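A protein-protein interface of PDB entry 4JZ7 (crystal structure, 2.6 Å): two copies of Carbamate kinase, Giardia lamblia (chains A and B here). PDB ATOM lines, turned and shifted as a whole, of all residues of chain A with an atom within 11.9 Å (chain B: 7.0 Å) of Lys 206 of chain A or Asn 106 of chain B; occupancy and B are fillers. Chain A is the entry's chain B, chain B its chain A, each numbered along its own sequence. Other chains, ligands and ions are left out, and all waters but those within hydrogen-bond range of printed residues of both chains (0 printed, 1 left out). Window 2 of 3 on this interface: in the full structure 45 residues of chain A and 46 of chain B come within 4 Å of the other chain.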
ATOM      1  N   GLN A 117      15.497 -22.141   0.938  1.00  0.00           N
ATOM      2  CA  GLN A 117      15.335 -21.320   2.135  1.00  0.00           C
ATOM      3  C   GLN A 117      15.249 -22.218   3.353  1.00  0.00           C
ATOM      4  O   GLN A 117      14.770 -23.347   3.262  1.00  0.00           O
ATOM      5  CB  GLN A 117      14.073 -20.448   2.042  1.00  0.00           C
ATOM      6  CG  GLN A 117      14.005 -19.533   0.817  1.00  0.00           C
ATOM      7  CD  GLN A 117      12.633 -18.896   0.624  1.00  0.00           C
ATOM      8  OE1 GLN A 117      12.389 -17.771   1.071  1.00  0.00           O
ATOM      9  NE2 GLN A 117      11.729 -19.615  -0.044  1.00  0.00           N
ATOM     10  N   LEU A 119      13.963 -22.093   7.406  1.00  0.00           N
ATOM     11  CA  LEU A 119      13.356 -21.451   8.561  1.00  0.00           C
ATOM     12  C   LEU A 119      14.191 -21.663   9.826  1.00  0.00           C
ATOM     13  O   LEU A 119      14.748 -22.745  10.039  1.00  0.00           O
ATOM     14  CB  LEU A 119      11.930 -21.988   8.766  1.00  0.00           C
ATOM     15  CG  LEU A 119      10.970 -21.673   7.609  1.00  0.00           C
ATOM     16  CD1 LEU A 119       9.586 -22.293   7.787  1.00  0.00           C
ATOM     17  CD2 LEU A 119      10.871 -20.175   7.397  1.00  0.00           C
ATOM     18  N   PRO A 122      13.810 -16.856  15.247  1.00  0.00           N
ATOM     19  CA  PRO A 122      14.587 -15.606  15.184  1.00  0.00           C
ATOM     20  C   PRO A 122      15.130 -15.117  16.549  1.00  0.00           C
ATOM     21  O   PRO A 122      15.966 -14.200  16.587  1.00  0.00           O
ATOM     22  CB  PRO A 122      13.579 -14.603  14.588  1.00  0.00           C
ATOM     23  CG  PRO A 122      12.239 -15.115  15.037  1.00  0.00           C
ATOM     24  CD  PRO A 122      12.360 -16.624  15.083  1.00  0.00           C
ATOM     25  N   GLU A 174      13.230 -25.714   9.352  1.00  0.00           N
ATOM     26  CA  GLU A 174      12.516 -26.189   8.178  1.00  0.00           C
ATOM     27  C   GLU A 174      13.197 -25.812   6.862  1.00  0.00           C
ATOM     28  O   GLU A 174      13.552 -24.658   6.641  1.00  0.00           O
ATOM     29  CB  GLU A 174      11.072 -25.672   8.187  1.00  0.00           C
ATOM     30  CG  GLU A 174      10.073 -26.575   7.439  1.00  0.00           C
ATOM     31  CD  GLU A 174       8.702 -25.923   7.217  1.00  0.00           C
ATOM     32  OE1 GLU A 174       8.325 -25.711   6.037  1.00  0.00           O
ATOM     33  OE2 GLU A 174       7.999 -25.635   8.216  1.00  0.00           O
ATOM     34  N   VAL A 176      12.230 -25.003   3.321  1.00  0.00           N
ATOM     35  CA  VAL A 176      10.952 -24.607   2.724  1.00  0.00           C
ATOM     36  C   VAL A 176      10.633 -25.469   1.509  1.00  0.00           C
ATOM     37  O   VAL A 176       9.492 -25.949   1.359  1.00  0.00           O
ATOM     38  CB  VAL A 176      10.916 -23.104   2.319  1.00  0.00           C
ATOM     39  CG1 VAL A 176       9.748 -22.824   1.386  1.00  0.00           C
ATOM     40  CG2 VAL A 176      10.833 -22.209   3.565  1.00  0.00           C
ATOM     41  N   CYS A 201      15.884 -17.884   7.095  1.00  0.00           N
ATOM     42  CA  CYS A 201      14.611 -17.180   7.084  1.00  0.00           C
ATOM     43  C   CYS A 201      13.833 -17.455   8.357  1.00  0.00           C
ATOM     44  O   CYS A 201      14.218 -18.299   9.174  1.00  0.00           O
ATOM     45  CB  CYS A 201      13.771 -17.652   5.911  1.00  0.00           C
ATOM     46  SG  CYS A 201      14.465 -17.217   4.290  1.00  0.00           S
ATOM     47  N   LYS A 202      12.709 -16.759   8.507  1.00  0.00           N
ATOM     48  CA  LYS A 202      11.794 -16.988   9.620  1.00  0.00           C
ATOM     49  C   LYS A 202      10.393 -16.643   9.161  1.00  0.00           C
ATOM     50  O   LYS A 202      10.216 -15.897   8.206  1.00  0.00           O
ATOM     51  CB  LYS A 202      12.161 -16.119  10.818  1.00  0.00           C
ATOM     52  CG  LYS A 202      11.363 -14.832  10.877  1.00  0.00           C
ATOM     53  CD  LYS A 202      12.289 -13.644  10.868  1.00  0.00           C
ATOM     54  CE  LYS A 202      11.571 -12.413  10.339  1.00  0.00           C
ATOM     55  NZ  LYS A 202      12.491 -11.615   9.485  1.00  0.00           N
ATOM     56  N   ARG A 203       9.396 -17.174   9.849  1.00  0.00           N
ATOM     57  CA  ARG A 203       8.020 -17.032   9.394  1.00  0.00           C
ATOM     58  C   ARG A 203       7.087 -16.518  10.503  1.00  0.00           C
ATOM     59  O   ARG A 203       6.590 -17.299  11.320  1.00  0.00           O
ATOM     60  CB  ARG A 203       7.530 -18.378   8.855  1.00  0.00           C
ATOM     61  CG  ARG A 203       6.279 -18.285   8.015  1.00  0.00           C
ATOM     62  CD  ARG A 203       5.282 -19.380   8.387  1.00  0.00           C
ATOM     63  NE  ARG A 203       5.826 -20.713   8.161  1.00  0.00           N
ATOM     64  CZ  ARG A 203       5.993 -21.253   6.958  1.00  0.00           C
ATOM     65  NH1 ARG A 203       5.673 -20.558   5.866  1.00  0.00           N
ATOM     66  NH2 ARG A 203       6.483 -22.485   6.846  1.00  0.00           N
ATOM     67  N   GLU A 204       6.836 -15.207  10.499  1.00  0.00           N
ATOM     68  CA  GLU A 204       5.928 -14.587  11.465  1.00  0.00           C
ATOM     69  C   GLU A 204       4.587 -14.238  10.827  1.00  0.00           C
ATOM     70  O   GLU A 204       4.518 -13.474   9.862  1.00  0.00           O
ATOM     71  CB  GLU A 204       6.545 -13.324  12.087  1.00  0.00           C
ATOM     72  CG  GLU A 204       7.998 -13.080  11.737  1.00  0.00           C
ATOM     73  CD  GLU A 204       8.858 -12.769  12.963  1.00  0.00           C
ATOM     74  OE1 GLU A 204       9.612 -11.759  12.934  1.00  0.00           O
ATOM     75  OE2 GLU A 204       8.794 -13.552  13.944  1.00  0.00           O
ATOM     76  N   ASN A 205       3.515 -14.786  11.385  1.00  0.00           N
ATOM     77  CA  ASN A 205       2.180 -14.435  10.931  1.00  0.00           C
ATOM     78  C   ASN A 205       2.045 -14.596   9.420  1.00  0.00           C
ATOM     79  O   ASN A 205       1.681 -13.658   8.707  1.00  0.00           O
ATOM     80  CB  ASN A 205       1.827 -13.011  11.365  1.00  0.00           C
ATOM     81  CG  ASN A 205       0.334 -12.737  11.296  1.00  0.00           C
ATOM     82  OD1 ASN A 205      -0.466 -13.418  11.941  1.00  0.00           O
ATOM     83  ND2 ASN A 205      -0.049 -11.742  10.505  1.00  0.00           N
ATOM     84  N   LYS A 206       2.351 -15.800   8.941  1.00  0.00           N
ATOM     85  CA  LYS A 206       2.162 -16.153   7.537  1.00  0.00           C
ATOM     86  C   LYS A 206       3.144 -15.436   6.585  1.00  0.00           C
ATOM     87  O   LYS A 206       3.001 -15.507   5.365  1.00  0.00           O
ATOM     88  CB  LYS A 206       0.688 -15.949   7.143  1.00  0.00           C
ATOM     89  CG  LYS A 206      -0.255 -17.023   7.734  1.00  0.00           C
ATOM     90  CD  LYS A 206      -1.716 -16.530   7.881  1.00  0.00           C
ATOM     91  CE  LYS A 206      -2.365 -16.182   6.542  1.00  0.00           C
ATOM     92  NZ  LYS A 206      -3.713 -16.812   6.355  1.00  0.00           N
ATOM     93  N   VAL A 207       4.161 -14.789   7.146  1.00  0.00           N
ATOM     94  CA  VAL A 207       5.142 -14.092   6.319  1.00  0.00           C
ATOM     95  C   VAL A 207       6.582 -14.537   6.571  1.00  0.00           C
ATOM     96  O   VAL A 207       7.142 -14.328   7.665  1.00  0.00           O
ATOM     97  CB  VAL A 207       5.032 -12.555   6.464  1.00  0.00           C
ATOM     98  CG1 VAL A 207       5.972 -11.849   5.471  1.00  0.00           C
ATOM     99  CG2 VAL A 207       3.595 -12.120   6.237  1.00  0.00           C
ATOM    100  N   ILE A 208       7.163 -15.153   5.539  1.00  0.00           N
ATOM    101  CA  ILE A 208       8.569 -15.518   5.548  1.00  0.00           C
ATOM    102  C   ILE A 208       9.368 -14.322   5.093  1.00  0.00           C
ATOM    103  O   ILE A 208       9.034 -13.683   4.101  1.00  0.00           O
ATOM    104  CB  ILE A 208       8.873 -16.654   4.567  1.00  0.00           C
ATOM    105  CG1 ILE A 208       8.153 -17.942   4.969  1.00  0.00           C
ATOM    106  CG2 ILE A 208      10.384 -16.897   4.486  1.00  0.00           C
ATOM    107  CD1 ILE A 208       8.309 -19.063   3.913  1.00  0.00           C
ATOM    108  N   SER A 209      10.423 -14.030   5.835  1.00  0.00           N
ATOM    109  CA  SER A 209      11.288 -12.904   5.551  1.00  0.00           C
ATOM    110  C   SER A 209      12.687 -13.397   5.856  1.00  0.00           C
ATOM    111  O   SER A 209      12.854 -14.382   6.570  1.00  0.00           O
ATOM    112  CB  SER A 209      10.914 -11.732   6.455  1.00  0.00           C
ATOM    113  OG  SER A 209      11.994 -11.333   7.277  1.00  0.00           O
ATOM    114  N   GLY A 210      13.698 -12.736   5.315  1.00  0.00           N
ATOM    115  CA  GLY A 210      15.059 -13.171   5.570  1.00  0.00           C
ATOM    116  C   GLY A 210      15.726 -12.570   6.803  1.00  0.00           C
ATOM    117  O   GLY A 210      15.703 -11.350   7.021  1.00  0.00           O
ATOM    118  N   TYR B  41      -0.366 -14.985  -8.476  1.00  0.00           N
ATOM    119  CA  TYR B  41      -1.171 -15.926  -7.690  1.00  0.00           C
ATOM    120  C   TYR B  41      -2.554 -16.096  -8.299  1.00  0.00           C
ATOM    121  O   TYR B  41      -3.080 -17.200  -8.371  1.00  0.00           O
ATOM    122  CB  TYR B  41      -1.327 -15.480  -6.238  1.00  0.00           C
ATOM    123  CG  TYR B  41      -2.097 -16.505  -5.444  1.00  0.00           C
ATOM    124  CD1 TYR B  41      -1.509 -17.712  -5.095  1.00  0.00           C
ATOM    125  CD2 TYR B  41      -3.428 -16.298  -5.086  1.00  0.00           C
ATOM    126  CE1 TYR B  41      -2.213 -18.671  -4.393  1.00  0.00           C
ATOM    127  CE2 TYR B  41      -4.137 -17.259  -4.387  1.00  0.00           C
ATOM    128  CZ  TYR B  41      -3.517 -18.436  -4.048  1.00  0.00           C
ATOM    129  OH  TYR B  41      -4.190 -19.401  -3.356  1.00  0.00           O
ATOM    130  N   ASP B  99       5.621 -17.904  -2.215  1.00  0.00           N
ATOM    131  CA  ASP B  99       5.234 -18.700  -1.058  1.00  0.00           C
ATOM    132  C   ASP B  99       4.369 -17.887  -0.101  1.00  0.00           C
ATOM    133  O   ASP B  99       3.340 -18.357   0.385  1.00  0.00           O
ATOM    134  CB  ASP B  99       6.464 -19.216  -0.315  1.00  0.00           C
ATOM    135  CG  ASP B  99       7.165 -20.349  -1.051  1.00  0.00           C
ATOM    136  OD1 ASP B  99       8.352 -20.619  -0.749  1.00  0.00           O
ATOM    137  OD2 ASP B  99       6.529 -20.968  -1.934  1.00  0.00           O
ATOM    138  N   ASN B 100       4.785 -16.654   0.165  1.00  0.00           N
ATOM    139  CA  ASN B 100       4.027 -15.779   1.060  1.00  0.00           C
ATOM    140  C   ASN B 100       2.636 -15.461   0.554  1.00  0.00           C
ATOM    141  O   ASN B 100       1.704 -15.347   1.353  1.00  0.00           O
ATOM    142  CB  ASN B 100       4.777 -14.467   1.325  1.00  0.00           C
ATOM    143  CG  ASN B 100       6.029 -14.673   2.146  1.00  0.00           C
ATOM    144  OD1 ASN B 100       6.101 -15.587   2.961  1.00  0.00           O
ATOM    145  ND2 ASN B 100       7.028 -13.827   1.927  1.00  0.00           N
ATOM    146  N   VAL B 101       2.480 -15.316  -0.760  1.00  0.00           N
ATOM    147  CA  VAL B 101       1.133 -15.065  -1.298  1.00  0.00           C
ATOM    148  C   VAL B 101       0.292 -16.344  -1.252  1.00  0.00           C
ATOM    149  O   VAL B 101      -0.905 -16.301  -1.010  1.00  0.00           O
ATOM    150  CB  VAL B 101       1.174 -14.418  -2.706  1.00  0.00           C
ATOM    151  CG1 VAL B 101       1.473 -15.472  -3.786  1.00  0.00           C
ATOM    152  CG2 VAL B 101      -0.126 -13.695  -2.992  1.00  0.00           C
ATOM    153  N   PHE B 102       0.939 -17.490  -1.432  1.00  0.00           N
ATOM    154  CA  PHE B 102       0.291 -18.775  -1.204  1.00  0.00           C
ATOM    155  C   PHE B 102      -0.281 -18.880   0.201  1.00  0.00           C
ATOM    156  O   PHE B 102      -1.501 -18.946   0.385  1.00  0.00           O
ATOM    157  CB  PHE B 102       1.266 -19.929  -1.428  1.00  0.00           C
ATOM    158  CG  PHE B 102       1.286 -20.441  -2.838  1.00  0.00           C
ATOM    159  CD1 PHE B 102       1.687 -19.624  -3.882  1.00  0.00           C
ATOM    160  CD2 PHE B 102       0.916 -21.740  -3.117  1.00  0.00           C
ATOM    161  CE1 PHE B 102       1.718 -20.084  -5.181  1.00  0.00           C
ATOM    162  CE2 PHE B 102       0.942 -22.215  -4.418  1.00  0.00           C
ATOM    163  CZ  PHE B 102       1.347 -21.380  -5.454  1.00  0.00           C
ATOM    164  N   CYS B 103       0.612 -18.907   1.185  1.00  0.00           N
ATOM    165  CA  CYS B 103       0.210 -19.006   2.587  1.00  0.00           C
ATOM    166  C   CYS B 103      -0.871 -17.963   2.936  1.00  0.00           C
ATOM    167  O   CYS B 103      -1.865 -18.287   3.592  1.00  0.00           O
ATOM    168  CB  CYS B 103       1.437 -18.880   3.495  1.00  0.00           C
ATOM    169  SG  CYS B 103       1.126 -19.080   5.281  1.00  0.00           S
ATOM    170  N   ALA B 104      -0.690 -16.729   2.472  1.00  0.00           N
ATOM    171  CA  ALA B 104      -1.691 -15.694   2.694  1.00  0.00           C
ATOM    172  C   ALA B 104      -3.084 -16.223   2.337  1.00  0.00           C
ATOM    173  O   ALA B 104      -4.076 -15.867   2.965  1.00  0.00           O
ATOM    174  CB  ALA B 104      -1.358 -14.469   1.880  1.00  0.00           C
ATOM    175  N   ASN B 105      -3.141 -17.096   1.335  1.00  0.00           N
ATOM    176  CA  ASN B 105      -4.391 -17.684   0.875  1.00  0.00           C
ATOM    177  C   ASN B 105      -4.622 -19.091   1.406  1.00  0.00           C
ATOM    178  O   ASN B 105      -5.435 -19.842   0.860  1.00  0.00           O
ATOM    179  CB  ASN B 105      -4.444 -17.723  -0.650  1.00  0.00           C
ATOM    180  CG  ASN B 105      -4.793 -16.387  -1.247  1.00  0.00           C
ATOM    181  OD1 ASN B 105      -5.923 -16.165  -1.691  1.00  0.00           O
ATOM    182  ND2 ASN B 105      -3.826 -15.478  -1.260  1.00  0.00           N
ATOM    183  N   ASN B 106      -3.888 -19.465   2.448  1.00  0.00           N
ATOM    184  CA  ASN B 106      -4.129 -20.750   3.091  1.00  0.00           C
ATOM    185  C   ASN B 106      -3.925 -21.946   2.149  1.00  0.00           C
ATOM    186  O   ASN B 106      -4.519 -23.010   2.332  1.00  0.00           O
ATOM    187  CB  ASN B 106      -5.533 -20.776   3.721  1.00  0.00           C
ATOM    188  CG  ASN B 106      -5.703 -19.714   4.806  1.00  0.00           C
ATOM    189  OD1 ASN B 106      -4.894 -19.632   5.738  1.00  0.00           O
ATOM    190  ND2 ASN B 106      -6.734 -18.871   4.668  1.00  0.00           N
ATOM    191  N   GLU B 107      -3.105 -21.753   1.122  1.00  0.00           N
ATOM    192  CA  GLU B 107      -2.694 -22.854   0.265  1.00  0.00           C
ATOM    193  C   GLU B 107      -1.241 -23.200   0.585  1.00  0.00           C
ATOM    194  O   GLU B 107      -0.392 -22.313   0.680  1.00  0.00           O
ATOM    195  CB  GLU B 107      -2.847 -22.479  -1.202  1.00  0.00           C
ATOM    196  CG  GLU B 107      -2.449 -23.583  -2.135  1.00  0.00           C
ATOM    197  CD  GLU B 107      -2.551 -23.169  -3.580  1.00  0.00           C
ATOM    198  OE1 GLU B 107      -2.008 -23.899  -4.438  1.00  0.00           O
ATOM    199  OE2 GLU B 107      -3.174 -22.117  -3.858  1.00  0.00           O
ATOM    200  N   PRO B 108      -0.957 -24.491   0.789  1.00  0.00           N
ATOM    201  CA  PRO B 108       0.414 -24.905   1.111  1.00  0.00           C
ATOM    202  C   PRO B 108       1.406 -24.533  -0.002  1.00  0.00           C
ATOM    203  O   PRO B 108       1.120 -24.692  -1.193  1.00  0.00           O
ATOM    204  CB  PRO B 108       0.308 -26.431   1.266  1.00  0.00           C
ATOM    205  CG  PRO B 108      -0.991 -26.809   0.631  1.00  0.00           C
ATOM    206  CD  PRO B 108      -1.893 -25.628   0.772  1.00  0.00           C
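The side-chain amide oxygen (OD1) of Asn 100 of chain B is in hydrogen-bond range of the backbone NH (N) of Ile 208 of chain A (2.8 Å). The side-chain amide oxygen of Asn 106 of chain B lies within hydrogen-bond range of the side-chain amino group of Lys 206 of chain A (3.1 Å).
The backbone NH (N) of Val 176 of chain A is in hydrogen-bond range of the backbone carbonyl oxygen (O) of Gln 117 of chain A.
Gln 117 of chain A touches Asp 99 of chain B (NE2 to OD1, 3.6 Å). OD1 of Asp 99 of chain B touches CG1 of Val 176 of chain A (3.4 Å). O of Lys 206 of chain A touches OD1 of Asn 100 of chain B (3.9 Å). CG of Lys 206 of chain A touches SG of Cys 103 of chain B (3.5 Å). Ala 104 of chain B touches Lys 206 of chain A (O to NZ, 3.5 Å). C of Val 207 of chain A touches OD1 of Asn 100 of chain B (3.8 Å).
Lys 206 of chain A touches four residues of chain B. Asn 100 of chain B touches just these residues of chain A: Lys 206, Val 207 and Ile 208. Of chain A, only Lys 206 comes within 4 Å of Cys 103 of chain B. Ala 104 of chain B touches just one residue of chain A: Lys 206. No residue of chain A comes within 4 Å of Asn 105 of chain B. No residue of chain A comes within 4 Å of Glu 107 of chain B. No residue of chain A comes within 4 Å of Pro 108 of chain B. Of the printed residues of chain A, Asp 99 of chain B touches Gln 117 (3.6 Å) and Val 176 (3.4 Å). Printed residues of chain B within 4 Å of Ile 208 of chain A: Asn 100. The nearest residue of chain B that does not touch Lys 206 of chain A is Asn 105 of chain B (5.1 Å). The nearest residue of chain A that does not touch Asn 106 of chain B is Asn 205 of chain A (9.3 Å). The nearest printed residue of chain B that does not touch Val 176 of chain A is Asn 100 of chain B (8.0 Å).
Printed residues of chain A that touch a printed residue of chain B: Gln 117, Val 176, Lys 206, Val 207 and Ile 208. Hydrophobic or aromatic side chains of chain A that line the printed part of chain B: Val 176 and Ile 208. Among the printed residues, no Asp or Glu carboxylate lies within 4 Å of a Lys or Arg side-chain nitrogen of the other chain.
No position is printed for both chains. Of the 8 pairs that touch across the chains among the printed residues, none has its exchanged pair printed and touching as well.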
